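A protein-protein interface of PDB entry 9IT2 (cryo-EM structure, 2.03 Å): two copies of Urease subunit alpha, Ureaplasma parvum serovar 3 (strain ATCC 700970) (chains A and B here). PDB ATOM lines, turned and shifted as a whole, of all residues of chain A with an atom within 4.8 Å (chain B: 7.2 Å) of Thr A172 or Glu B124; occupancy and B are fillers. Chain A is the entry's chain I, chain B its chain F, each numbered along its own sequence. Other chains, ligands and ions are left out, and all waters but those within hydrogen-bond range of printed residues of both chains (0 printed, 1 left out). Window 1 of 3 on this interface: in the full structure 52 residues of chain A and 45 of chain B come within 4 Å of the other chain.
Trp A144 touches Phe B483.
Phe B483 touches Gly A167 (CD2 to CA, 3.96 Å).
Asn A169 touches Ser B126 (OD1 to CB, 3.4 Å).
Asp A170 touches Ile B125 (N to O, 3.6 Å).
Gly A171 touches Phe B45 (CA to CE2, 3.5 Å).
Ala A174 touches Phe B45.
CG of Pro A179 touches O of Thr B123, 3.6 Å away.
CG of Pro A179 touches N of Glu B124 (3.9 Å).
CZ3 of Trp A228 touches CE1 of Phe B45, at 3.5 Å.
Trp A228 touches Ile B125 (CH2 to CG1, 3.9 Å).
Printed residues of chain A that touch a printed residue of chain B: Trp A144, Leu A145, Thr A166, Gly A167, Asn A169, Asp A170, Gly A171, Thr A172, Ala A174, Pro A179, Trp A183 and Trp A228.
Hydrophobic or aromatic side chains of chain A that line the printed part of chain B: Trp A144, Ala A174, Pro A179, Trp A183 and Trp A228.
Of the 18 printed residues of chain B, 9 touch a printed residue of chain A.
Hydrophobic or aromatic side chains of chain B that line the printed part of chain A: Phe B45, Ile B125 and Phe B483.
Along chain B the printed residues that touch a printed residue of chain A span positions 45 to 483.
No position is printed for both chains.
Of the 24 pairs that touch across the chains among the printed residues, none has its exchanged pair printed and touching as well.
Of chain B, only Glu B124 (2.9 Å) comes within 4 Å of Thr A172.
Of the printed residues of chain A, Glu B124 touches Thr A166, Asn A169, Gly A171, Thr A172, Pro A179 and Trp A183.
Printed residues of chain B within 4 Å of Trp A228: Phe B45 (3.5 Å), Thr B123 (3.6 Å) and Ile B125 (3.9 Å).
Of the printed residues of chain B, Gly A167 touches Phe B483 (3.96 Å).
Val A177 touches none of the printed residues of chain B.
Gly A165 touches none of the printed residues of chain B.
The nearest residue of chain B that does not touch Thr A172 is Ile B125 (5.2 Å).
The nearest printed residue of chain A that does not touch Ile B125 is Thr A172 (5.2 Å).
The backbone carbonyl oxygen (O) of Met B73 lies within hydrogen-bond range of the side-chain hydroxyl (OG1) of Thr B123.
O of Asp B74 sits at hydrogen-bond distance from N of Glu B124, 2.9 Å away.
The backbone NH (N) of Ser B126 sits at hydrogen-bond distance from the backbone carbonyl oxygen (O) of Val B76 (2.9 Å).
ND1 of His A143 lies within hydrogen-bond range of O of Thr A172.
The backbone carbonyl oxygen of Trp A144 sits at hydrogen-bond distance from the backbone NH of Gly A167.
The backbone NH (N) of Thr A166 lies within hydrogen-bond range of the side-chain hydroxyl (OG1) of Thr A172 (2.6 Å).
O of Asp B74 sits at hydrogen-bond distance from NE1 of Trp A183 (2.9 Å).
The side-chain carboxylate of Glu B124 lies within hydrogen-bond range of the side-chain hydroxyl of Thr A166, 2.4 Å away.
The side-chain hydroxyl (OG1) of Thr A172 lies within hydrogen-bond range of the side-chain carboxylate (OE2) of Glu B124 (2.9 Å).
The backbone NH (N) of Gly A171 lies within hydrogen-bond range of the backbone carbonyl oxygen (O) of Ile B125, 3.0 Å away.
The backbone carbonyl oxygen (O) of Pro A179 sits close to the backbone carbonyl oxygen (O) of Ser B122, at 3.4 Å.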
ATOM      1  N   HIS A 143      -8.549 -26.259  -3.703  1.00  0.00           N
ATOM      2  CA  HIS A 143      -8.117 -24.884  -3.916  1.00  0.00           C
ATOM      3  C   HIS A 143      -9.080 -24.225  -4.898  1.00  0.00           C
ATOM      4  O   HIS A 143      -9.266 -24.715  -6.017  1.00  0.00           O
ATOM      5  CB  HIS A 143      -6.681 -24.833  -4.438  1.00  0.00           C
ATOM      6  CG  HIS A 143      -5.661 -25.305  -3.447  1.00  0.00           C
ATOM      7  ND1 HIS A 143      -4.750 -24.456  -2.857  1.00  0.00           N
ATOM      8  CD2 HIS A 143      -5.402 -26.538  -2.952  1.00  0.00           C
ATOM      9  CE1 HIS A 143      -3.978 -25.144  -2.034  1.00  0.00           C
ATOM     10  NE2 HIS A 143      -4.354 -26.410  -2.072  1.00  0.00           N
ATOM     11  N   TRP A 144      -9.694 -23.122  -4.473  1.00  0.00           N
ATOM     12  CA  TRP A 144     -10.726 -22.433  -5.250  1.00  0.00           C
ATOM     13  C   TRP A 144     -10.032 -21.587  -6.316  1.00  0.00           C
ATOM     14  O   TRP A 144      -9.845 -20.376  -6.179  1.00  0.00           O
ATOM     15  CB  TRP A 144     -11.597 -21.595  -4.321  1.00  0.00           C
ATOM     16  CG  TRP A 144     -12.860 -21.049  -4.919  1.00  0.00           C
ATOM     17  CD1 TRP A 144     -13.112 -19.753  -5.258  1.00  0.00           C
ATOM     18  CD2 TRP A 144     -14.061 -21.778  -5.202  1.00  0.00           C
ATOM     19  NE1 TRP A 144     -14.386 -19.633  -5.755  1.00  0.00           N
ATOM     20  CE2 TRP A 144     -14.992 -20.861  -5.727  1.00  0.00           C
ATOM     21  CE3 TRP A 144     -14.437 -23.118  -5.071  1.00  0.00           C
ATOM     22  CZ2 TRP A 144     -16.273 -21.240  -6.123  1.00  0.00           C
ATOM     23  CZ3 TRP A 144     -15.709 -23.492  -5.464  1.00  0.00           C
ATOM     24  CH2 TRP A 144     -16.611 -22.558  -5.984  1.00  0.00           C
ATOM     25  N   LEU A 145      -9.644 -22.249  -7.407  1.00  0.00           N
ATOM     26  CA  LEU A 145      -8.781 -21.650  -8.419  1.00  0.00           C
ATOM     27  C   LEU A 145      -9.501 -21.320  -9.720  1.00  0.00           C
ATOM     28  O   LEU A 145      -9.409 -20.184 -10.197  1.00  0.00           O
ATOM     29  CB  LEU A 145      -7.587 -22.576  -8.699  1.00  0.00           C
ATOM     30  CG  LEU A 145      -6.439 -22.446  -7.692  1.00  0.00           C
ATOM     31  CD1 LEU A 145      -5.516 -23.644  -7.746  1.00  0.00           C
ATOM     32  CD2 LEU A 145      -5.655 -21.169  -7.935  1.00  0.00           C
ATOM     33  N   GLY A 164     -11.403 -23.430  -0.494  1.00  0.00           N
ATOM     34  CA  GLY A 164     -10.881 -22.179   0.012  1.00  0.00           C
ATOM     35  C   GLY A 164      -9.978 -21.523  -1.010  1.00  0.00           C
ATOM     36  O   GLY A 164      -9.146 -22.195  -1.625  1.00  0.00           O
ATOM     37  N   GLY A 165     -10.132 -20.228  -1.213  1.00  0.00           N
ATOM     38  CA  GLY A 165      -9.298 -19.529  -2.169  1.00  0.00           C
ATOM     39  C   GLY A 165     -10.003 -18.314  -2.737  1.00  0.00           C
ATOM     40  O   GLY A 165     -11.113 -17.965  -2.346  1.00  0.00           O
ATOM     41  N   THR A 166      -9.315 -17.679  -3.690  1.00  0.00           N
ATOM     42  CA  THR A 166      -9.726 -16.395  -4.245  1.00  0.00           C
ATOM     43  C   THR A 166      -9.682 -16.370  -5.768  1.00  0.00           C
ATOM     44  O   THR A 166      -9.773 -15.288  -6.359  1.00  0.00           O
ATOM     45  CB  THR A 166      -8.834 -15.269  -3.707  1.00  0.00           C
ATOM     46  OG1 THR A 166      -7.489 -15.470  -4.160  1.00  0.00           O
ATOM     47  CG2 THR A 166      -8.847 -15.247  -2.193  1.00  0.00           C
ATOM     48  N   GLY A 167      -9.550 -17.518  -6.415  1.00  0.00           N
ATOM     49  CA  GLY A 167      -9.251 -17.566  -7.827  1.00  0.00           C
ATOM     50  C   GLY A 167      -7.785 -17.852  -8.075  1.00  0.00           C
ATOM     51  O   GLY A 167      -7.080 -18.425  -7.242  1.00  0.00           O
ATOM     52  N   ASN A 169      -5.017 -16.494  -7.724  1.00  0.00           N
ATOM     53  CA  ASN A 169      -4.027 -15.716  -6.997  1.00  0.00           C
ATOM     54  C   ASN A 169      -3.021 -16.658  -6.346  1.00  0.00           C
ATOM     55  O   ASN A 169      -3.344 -17.798  -6.001  1.00  0.00           O
ATOM     56  CB  ASN A 169      -4.687 -14.832  -5.936  1.00  0.00           C
ATOM     57  CG  ASN A 169      -5.356 -13.607  -6.529  1.00  0.00           C
ATOM     58  OD1 ASN A 169      -4.738 -12.849  -7.276  1.00  0.00           O
ATOM     59  ND2 ASN A 169      -6.624 -13.405  -6.196  1.00  0.00           N
ATOM     60  N   ASP A 170      -1.790 -16.167  -6.184  1.00  0.00           N
ATOM     61  CA  ASP A 170      -0.715 -17.006  -5.662  1.00  0.00           C
ATOM     62  C   ASP A 170      -1.006 -17.499  -4.250  1.00  0.00           C
ATOM     63  O   ASP A 170      -0.581 -18.600  -3.880  1.00  0.00           O
ATOM     64  CB  ASP A 170       0.605 -16.241  -5.710  1.00  0.00           C
ATOM     65  CG  ASP A 170       1.078 -16.002  -7.129  1.00  0.00           C
ATOM     66  OD1 ASP A 170       1.315 -14.833  -7.494  1.00  0.00           O
ATOM     67  OD2 ASP A 170       1.218 -16.990  -7.882  1.00  0.00           O
ATOM     68  N   GLY A 171      -1.723 -16.709  -3.450  1.00  0.00           N
ATOM     69  CA  GLY A 171      -2.136 -17.186  -2.141  1.00  0.00           C
ATOM     70  C   GLY A 171      -3.035 -18.404  -2.226  1.00  0.00           C
ATOM     71  O   GLY A 171      -2.913 -19.336  -1.427  1.00  0.00           O
ATOM     72  N   THR A 172      -3.948 -18.413  -3.198  1.00  0.00           N
ATOM     73  CA  THR A 172      -4.814 -19.568  -3.409  1.00  0.00           C
ATOM     74  C   THR A 172      -4.060 -20.719  -4.064  1.00  0.00           C
ATOM     75  O   THR A 172      -4.336 -21.890  -3.778  1.00  0.00           O
ATOM     76  CB  THR A 172      -6.020 -19.163  -4.257  1.00  0.00           C
ATOM     77  OG1 THR A 172      -6.791 -18.182  -3.551  1.00  0.00           O
ATOM     78  CG2 THR A 172      -6.896 -20.366  -4.574  1.00  0.00           C
ATOM     79  N   LYS A 173      -3.098 -20.406  -4.936  1.00  0.00           N
ATOM     80  CA  LYS A 173      -2.304 -21.453  -5.572  1.00  0.00           C
ATOM     81  C   LYS A 173      -1.543 -22.281  -4.546  1.00  0.00           C
ATOM     82  O   LYS A 173      -1.199 -23.438  -4.813  1.00  0.00           O
ATOM     83  CB  LYS A 173      -1.333 -20.836  -6.581  1.00  0.00           C
ATOM     84  CG  LYS A 173      -2.009 -20.217  -7.791  1.00  0.00           C
ATOM     85  CD  LYS A 173      -0.994 -19.623  -8.753  1.00  0.00           C
ATOM     86  CE  LYS A 173      -1.681 -18.842  -9.861  1.00  0.00           C
ATOM     87  NZ  LYS A 173      -0.706 -18.184 -10.773  1.00  0.00           N
ATOM     88  N   ALA A 174      -1.276 -21.712  -3.372  1.00  0.00           N
ATOM     89  CA  ALA A 174      -0.531 -22.402  -2.326  1.00  0.00           C
ATOM     90  C   ALA A 174      -1.431 -22.948  -1.224  1.00  0.00           C
ATOM     91  O   ALA A 174      -1.184 -24.047  -0.717  1.00  0.00           O
ATOM     92  CB  ALA A 174       0.513 -21.459  -1.721  1.00  0.00           C
ATOM     93  N   THR A 175      -2.467 -22.205  -0.839  1.00  0.00           N
ATOM     94  CA  THR A 175      -3.277 -22.531   0.327  1.00  0.00           C
ATOM     95  C   THR A 175      -4.758 -22.509  -0.033  1.00  0.00           C
ATOM     96  O   THR A 175      -5.184 -21.820  -0.962  1.00  0.00           O
ATOM     97  CB  THR A 175      -3.023 -21.548   1.483  1.00  0.00           C
ATOM     98  OG1 THR A 175      -3.809 -20.366   1.285  1.00  0.00           O
ATOM     99  CG2 THR A 175      -1.556 -21.155   1.555  1.00  0.00           C
ATOM    100  N   VAL A 177      -7.377 -20.993   1.316  1.00  0.00           N
ATOM    101  CA  VAL A 177      -7.729 -19.913   2.229  1.00  0.00           C
ATOM    102  C   VAL A 177      -8.534 -18.867   1.471  1.00  0.00           C
ATOM    103  O   VAL A 177      -8.044 -18.290   0.494  1.00  0.00           O
ATOM    104  CB  VAL A 177      -6.485 -19.272   2.865  1.00  0.00           C
ATOM    105  CG1 VAL A 177      -6.862 -17.987   3.579  1.00  0.00           C
ATOM    106  CG2 VAL A 177      -5.814 -20.244   3.824  1.00  0.00           C
ATOM    107  N   PRO A 179      -9.441 -15.464   2.498  1.00  0.00           N
ATOM    108  CA  PRO A 179      -9.149 -14.559   3.621  1.00  0.00           C
ATOM    109  C   PRO A 179     -10.171 -13.436   3.715  1.00  0.00           C
ATOM    110  O   PRO A 179     -10.370 -12.677   2.763  1.00  0.00           O
ATOM    111  CB  PRO A 179      -7.749 -14.020   3.292  1.00  0.00           C
ATOM    112  CG  PRO A 179      -7.410 -14.504   1.908  1.00  0.00           C
ATOM    113  CD  PRO A 179      -8.602 -15.186   1.324  1.00  0.00           C
ATOM    114  N   TRP A 183     -13.446 -12.102   0.466  1.00  0.00           N
ATOM    115  CA  TRP A 183     -13.174 -13.295  -0.323  1.00  0.00           C
ATOM    116  C   TRP A 183     -14.077 -14.457   0.066  1.00  0.00           C
ATOM    117  O   TRP A 183     -14.355 -15.325  -0.767  1.00  0.00           O
ATOM    118  CB  TRP A 183     -11.701 -13.677  -0.193  1.00  0.00           C
ATOM    119  CG  TRP A 183     -10.800 -12.696  -0.878  1.00  0.00           C
ATOM    120  CD1 TRP A 183      -9.907 -11.851  -0.287  1.00  0.00           C
ATOM    121  CD2 TRP A 183     -10.732 -12.429  -2.285  1.00  0.00           C
ATOM    122  NE1 TRP A 183      -9.274 -11.089  -1.237  1.00  0.00           N
ATOM    123  CE2 TRP A 183      -9.761 -11.426  -2.473  1.00  0.00           C
ATOM    124  CE3 TRP A 183     -11.391 -12.950  -3.403  1.00  0.00           C
ATOM    125  CZ2 TRP A 183      -9.434 -10.932  -3.734  1.00  0.00           C
ATOM    126  CZ3 TRP A 183     -11.062 -12.459  -4.653  1.00  0.00           C
ATOM    127  CH2 TRP A 183     -10.094 -11.460  -4.809  1.00  0.00           C
ATOM    128  N   TRP A 228       1.125 -19.303   5.364  1.00  0.00           N
ATOM    129  CA  TRP A 228       0.677 -18.181   6.176  1.00  0.00           C
ATOM    130  C   TRP A 228       1.288 -18.195   7.571  1.00  0.00           C
ATOM    131  O   TRP A 228       1.109 -17.231   8.322  1.00  0.00           O
ATOM    132  CB  TRP A 228      -0.853 -18.185   6.289  1.00  0.00           C
ATOM    133  CG  TRP A 228      -1.557 -17.932   4.989  1.00  0.00           C
ATOM    134  CD1 TRP A 228      -2.326 -18.816   4.289  1.00  0.00           C
ATOM    135  CD2 TRP A 228      -1.556 -16.715   4.230  1.00  0.00           C
ATOM    136  NE1 TRP A 228      -2.804 -18.226   3.146  1.00  0.00           N
ATOM    137  CE2 TRP A 228      -2.345 -16.936   3.085  1.00  0.00           C
ATOM    138  CE3 TRP A 228      -0.963 -15.462   4.409  1.00  0.00           C
ATOM    139  CZ2 TRP A 228      -2.558 -15.951   2.124  1.00  0.00           C
ATOM    140  CZ3 TRP A 228      -1.176 -14.485   3.454  1.00  0.00           C
ATOM    141  CH2 TRP A 228      -1.967 -14.735   2.325  1.00  0.00           C
ATOM    142  N   PHE B  45       5.417 -13.771  -0.645  1.00  0.00           N
ATOM    143  CA  PHE B  45       4.557 -14.798  -0.076  1.00  0.00           C
ATOM    144  C   PHE B  45       5.045 -16.182  -0.480  1.00  0.00           C
ATOM    145  O   PHE B  45       5.424 -16.405  -1.634  1.00  0.00           O
ATOM    146  CB  PHE B  45       3.105 -14.611  -0.523  1.00  0.00           C
ATOM    147  CG  PHE B  45       2.183 -15.690  -0.041  1.00  0.00           C
ATOM    148  CD1 PHE B  45       1.740 -15.705   1.270  1.00  0.00           C
ATOM    149  CD2 PHE B  45       1.766 -16.696  -0.896  1.00  0.00           C
ATOM    150  CE1 PHE B  45       0.895 -16.700   1.719  1.00  0.00           C
ATOM    151  CE2 PHE B  45       0.921 -17.694  -0.453  1.00  0.00           C
ATOM    152  CZ  PHE B  45       0.483 -17.695   0.856  1.00  0.00           C
ATOM    153  N   MET B  73      -5.738  -4.459   3.548  1.00  0.00           N
ATOM    154  CA  MET B  73      -6.206  -4.615   2.180  1.00  0.00           C
ATOM    155  C   MET B  73      -6.957  -5.927   2.002  1.00  0.00           C
ATOM    156  O   MET B  73      -6.724  -6.904   2.718  1.00  0.00           O
ATOM    157  CB  MET B  73      -5.031  -4.563   1.201  1.00  0.00           C
ATOM    158  CG  MET B  73      -4.257  -3.259   1.219  1.00  0.00           C
ATOM    159  SD  MET B  73      -5.232  -1.866   0.626  1.00  0.00           S
ATOM    160  CE  MET B  73      -5.452  -0.937   2.141  1.00  0.00           C
ATOM    161  N   ASP B  74      -7.875  -5.936   1.035  1.00  0.00           N
ATOM    162  CA  ASP B  74      -8.456  -7.199   0.593  1.00  0.00           C
ATOM    163  C   ASP B  74      -7.463  -7.984  -0.255  1.00  0.00           C
ATOM    164  O   ASP B  74      -7.376  -9.212  -0.141  1.00  0.00           O
ATOM    165  CB  ASP B  74      -9.747  -6.951  -0.189  1.00  0.00           C
ATOM    166  CG  ASP B  74     -10.864  -6.418   0.683  1.00  0.00           C
ATOM    167  OD1 ASP B  74     -10.939  -6.813   1.865  1.00  0.00           O
ATOM    168  OD2 ASP B  74     -11.670  -5.608   0.184  1.00  0.00           O
ATOM    169  N   LEU B  75      -6.706  -7.294  -1.106  1.00  0.00           N
ATOM    170  CA  LEU B  75      -5.731  -7.947  -1.969  1.00  0.00           C
ATOM    171  C   LEU B  75      -4.493  -7.070  -2.087  1.00  0.00           C
ATOM    172  O   LEU B  75      -4.597  -5.843  -2.112  1.00  0.00           O
ATOM    173  CB  LEU B  75      -6.324  -8.230  -3.357  1.00  0.00           C
ATOM    174  CG  LEU B  75      -5.390  -8.713  -4.470  1.00  0.00           C
ATOM    175  CD1 LEU B  75      -4.904 -10.128  -4.200  1.00  0.00           C
ATOM    176  CD2 LEU B  75      -6.085  -8.633  -5.820  1.00  0.00           C
ATOM    177  N   VAL B  76      -3.322  -7.697  -2.125  1.00  0.00           N
ATOM    178  CA  VAL B  76      -2.065  -6.986  -2.338  1.00  0.00           C
ATOM    179  C   VAL B  76      -1.302  -7.676  -3.458  1.00  0.00           C
ATOM    180  O   VAL B  76      -0.990  -8.868  -3.360  1.00  0.00           O
ATOM    181  CB  VAL B  76      -1.206  -6.914  -1.065  1.00  0.00           C
ATOM    182  CG1 VAL B  76       0.153  -6.306  -1.384  1.00  0.00           C
ATOM    183  CG2 VAL B  76      -1.908  -6.095   0.006  1.00  0.00           C
ATOM    184  N   ILE B  77      -1.007  -6.931  -4.517  1.00  0.00           N
ATOM    185  CA  ILE B  77      -0.121  -7.381  -5.584  1.00  0.00           C
ATOM    186  C   ILE B  77       1.276  -6.882  -5.241  1.00  0.00           C
ATOM    187  O   ILE B  77       1.525  -5.673  -5.209  1.00  0.00           O
ATOM    188  CB  ILE B  77      -0.579  -6.868  -6.954  1.00  0.00           C
ATOM    189  CG1 ILE B  77      -2.002  -7.344  -7.255  1.00  0.00           C
ATOM    190  CG2 ILE B  77       0.383  -7.321  -8.040  1.00  0.00           C
ATOM    191  CD1 ILE B  77      -2.649  -6.622  -8.414  1.00  0.00           C
ATOM    192  N   THR B  78       2.185  -7.815  -4.976  1.00  0.00           N
ATOM    193  CA  THR B  78       3.522  -7.480  -4.505  1.00  0.00           C
ATOM    194  C   THR B  78       4.503  -7.367  -5.664  1.00  0.00           C
ATOM    195  O   THR B  78       4.431  -8.129  -6.630  1.00  0.00           O
ATOM    196  CB  THR B  78       4.024  -8.529  -3.509  1.00  0.00           C
ATOM    197  OG1 THR B  78       4.147  -9.798  -4.165  1.00  0.00           O
ATOM    198  CG2 THR B  78       3.065  -8.656  -2.338  1.00  0.00           C
ATOM    199  N   ILE B  93       0.686  -2.888  -4.920  1.00  0.00           N
ATOM    200  CA  ILE B  93      -0.648  -2.358  -5.180  1.00  0.00           C
ATOM    201  C   ILE B  93      -1.608  -2.972  -4.172  1.00  0.00           C
ATOM    202  O   ILE B  93      -1.705  -4.198  -4.072  1.00  0.00           O
ATOM    203  CB  ILE B  93      -1.106  -2.644  -6.618  1.00  0.00           C
ATOM    204  CG1 ILE B  93      -0.093  -2.089  -7.622  1.00  0.00           C
ATOM    205  CG2 ILE B  93      -2.485  -2.055  -6.867  1.00  0.00           C
ATOM    206  CD1 ILE B  93      -0.240  -2.652  -9.014  1.00  0.00           C
ATOM    207  N   ILE B  95      -5.549  -3.292  -2.934  1.00  0.00           N
ATOM    208  CA  ILE B  95      -6.927  -3.193  -3.394  1.00  0.00           C
ATOM    209  C   ILE B  95      -7.851  -3.508  -2.225  1.00  0.00           C
ATOM    210  O   ILE B  95      -7.669  -4.519  -1.533  1.00  0.00           O
ATOM    211  CB  ILE B  95      -7.192  -4.153  -4.567  1.00  0.00           C
ATOM    212  CG1 ILE B  95      -6.321  -3.786  -5.771  1.00  0.00           C
ATOM    213  CG2 ILE B  95      -8.670  -4.162  -4.932  1.00  0.00           C
ATOM    214  CD1 ILE B  95      -6.079  -4.941  -6.716  1.00  0.00           C
ATOM    215  N   VAL B 119      -0.713  -5.885   5.186  1.00  0.00           N
ATOM    216  CA  VAL B 119      -1.093  -7.262   4.895  1.00  0.00           C
ATOM    217  C   VAL B 119      -1.616  -7.867   6.193  1.00  0.00           C
ATOM    218  O   VAL B 119      -0.858  -8.071   7.143  1.00  0.00           O
ATOM    219  CB  VAL B 119       0.085  -8.069   4.337  1.00  0.00           C
ATOM    220  CG1 VAL B 119      -0.326  -9.513   4.097  1.00  0.00           C
ATOM    221  CG2 VAL B 119       0.603  -7.432   3.056  1.00  0.00           C
ATOM    222  N   GLY B 120      -2.915  -8.140   6.242  1.00  0.00           N
ATOM    223  CA  GLY B 120      -3.521  -8.665   7.448  1.00  0.00           C
ATOM    224  C   GLY B 120      -4.098 -10.052   7.278  1.00  0.00           C
ATOM    225  O   GLY B 120      -3.905 -10.692   6.240  1.00  0.00           O
ATOM    226  N   ILE B 121      -4.812 -10.526   8.302  1.00  0.00           N
ATOM    227  CA  ILE B 121      -5.404 -11.861   8.262  1.00  0.00           C
ATOM    228  C   ILE B 121      -6.429 -11.966   7.141  1.00  0.00           C
ATOM    229  O   ILE B 121      -6.591 -13.029   6.530  1.00  0.00           O
ATOM    230  CB  ILE B 121      -6.019 -12.197   9.636  1.00  0.00           C
ATOM    231  CG1 ILE B 121      -4.935 -12.180  10.716  1.00  0.00           C
ATOM    232  CG2 ILE B 121      -6.716 -13.547   9.604  1.00  0.00           C
ATOM    233  CD1 ILE B 121      -3.733 -13.042  10.398  1.00  0.00           C
ATOM    234  N   SER B 122      -7.128 -10.873   6.845  1.00  0.00           N
ATOM    235  CA  SER B 122      -8.162 -10.847   5.821  1.00  0.00           C
ATOM    236  C   SER B 122      -7.627 -10.460   4.445  1.00  0.00           C
ATOM    237  O   SER B 122      -8.401 -10.002   3.597  1.00  0.00           O
ATOM    238  CB  SER B 122      -9.276  -9.886   6.241  1.00  0.00           C
ATOM    239  OG  SER B 122      -8.764  -8.584   6.451  1.00  0.00           O
ATOM    240  N   THR B 123      -6.332 -10.636   4.200  1.00  0.00           N
ATOM    241  CA  THR B 123      -5.691 -10.169   2.979  1.00  0.00           C
ATOM    242  C   THR B 123      -5.263 -11.344   2.107  1.00  0.00           C
ATOM    243  O   THR B 123      -4.680 -12.316   2.598  1.00  0.00           O
ATOM    244  CB  THR B 123      -4.471  -9.299   3.299  1.00  0.00           C
ATOM    245  OG1 THR B 123      -4.826  -8.314   4.276  1.00  0.00           O
ATOM    246  CG2 THR B 123      -3.962  -8.604   2.044  1.00  0.00           C
ATOM    247  N   GLU B 124      -5.555 -11.244   0.814  1.00  0.00           N
ATOM    248  CA  GLU B 124      -5.044 -12.163  -0.191  1.00  0.00           C
ATOM    249  C   GLU B 124      -3.830 -11.540  -0.872  1.00  0.00           C
ATOM    250  O   GLU B 124      -3.708 -10.315  -0.959  1.00  0.00           O
ATOM    251  CB  GLU B 124      -6.130 -12.502  -1.219  1.00  0.00           C
ATOM    252  CG  GLU B 124      -5.667 -13.274  -2.461  1.00  0.00           C
ATOM    253  CD  GLU B 124      -5.063 -14.639  -2.145  1.00  0.00           C
ATOM    254  OE1 GLU B 124      -3.996 -14.701  -1.498  1.00  0.00           O
ATOM    255  OE2 GLU B 124      -5.654 -15.659  -2.557  1.00  0.00           O
ATOM    256  N   ILE B 125      -2.914 -12.389  -1.333  1.00  0.00           N
ATOM    257  CA  ILE B 125      -1.653 -11.946  -1.914  1.00  0.00           C
ATOM    258  C   ILE B 125      -1.535 -12.485  -3.333  1.00  0.00           C
ATOM    259  O   ILE B 125      -1.799 -13.667  -3.580  1.00  0.00           O
ATOM    260  CB  ILE B 125      -0.448 -12.391  -1.063  1.00  0.00           C
ATOM    261  CG1 ILE B 125      -0.497 -11.721   0.311  1.00  0.00           C
ATOM    262  CG2 ILE B 125       0.857 -12.064  -1.770  1.00  0.00           C
ATOM    263  CD1 ILE B 125      -0.184 -10.242   0.279  1.00  0.00           C
ATOM    264  N   SER B 126      -1.149 -11.612  -4.262  1.00  0.00           N
ATOM    265  CA  SER B 126      -0.790 -11.989  -5.623  1.00  0.00           C
ATOM    266  C   SER B 126       0.638 -11.528  -5.881  1.00  0.00           C
ATOM    267  O   SER B 126       0.941 -10.338  -5.745  1.00  0.00           O
ATOM    268  CB  SER B 126      -1.754 -11.370  -6.639  1.00  0.00           C
ATOM    269  OG  SER B 126      -1.372 -11.678  -7.967  1.00  0.00           O
ATOM    270  N   PHE B 483     -13.956 -17.137 -11.797  1.00  0.00           N
ATOM    271  CA  PHE B 483     -15.099 -16.989 -10.902  1.00  0.00           C
ATOM    272  C   PHE B 483     -15.765 -15.626 -11.023  1.00  0.00           C
ATOM    273  O   PHE B 483     -16.939 -15.489 -10.662  1.00  0.00           O
ATOM    274  CB  PHE B 483     -14.669 -17.225  -9.453  1.00  0.00           C
ATOM    275  CG  PHE B 483     -14.172 -18.615  -9.190  1.00  0.00           C
ATOM    276  CD1 PHE B 483     -15.039 -19.694  -9.231  1.00  0.00           C
ATOM    277  CD2 PHE B 483     -12.839 -18.844  -8.896  1.00  0.00           C
ATOM    278  CE1 PHE B 483     -14.584 -20.974  -8.993  1.00  0.00           C
ATOM    279  CE2 PHE B 483     -12.380 -20.124  -8.652  1.00  0.00           C
ATOM    280  CZ  PHE B 483     -13.253 -21.190  -8.699  1.00  0.00           C
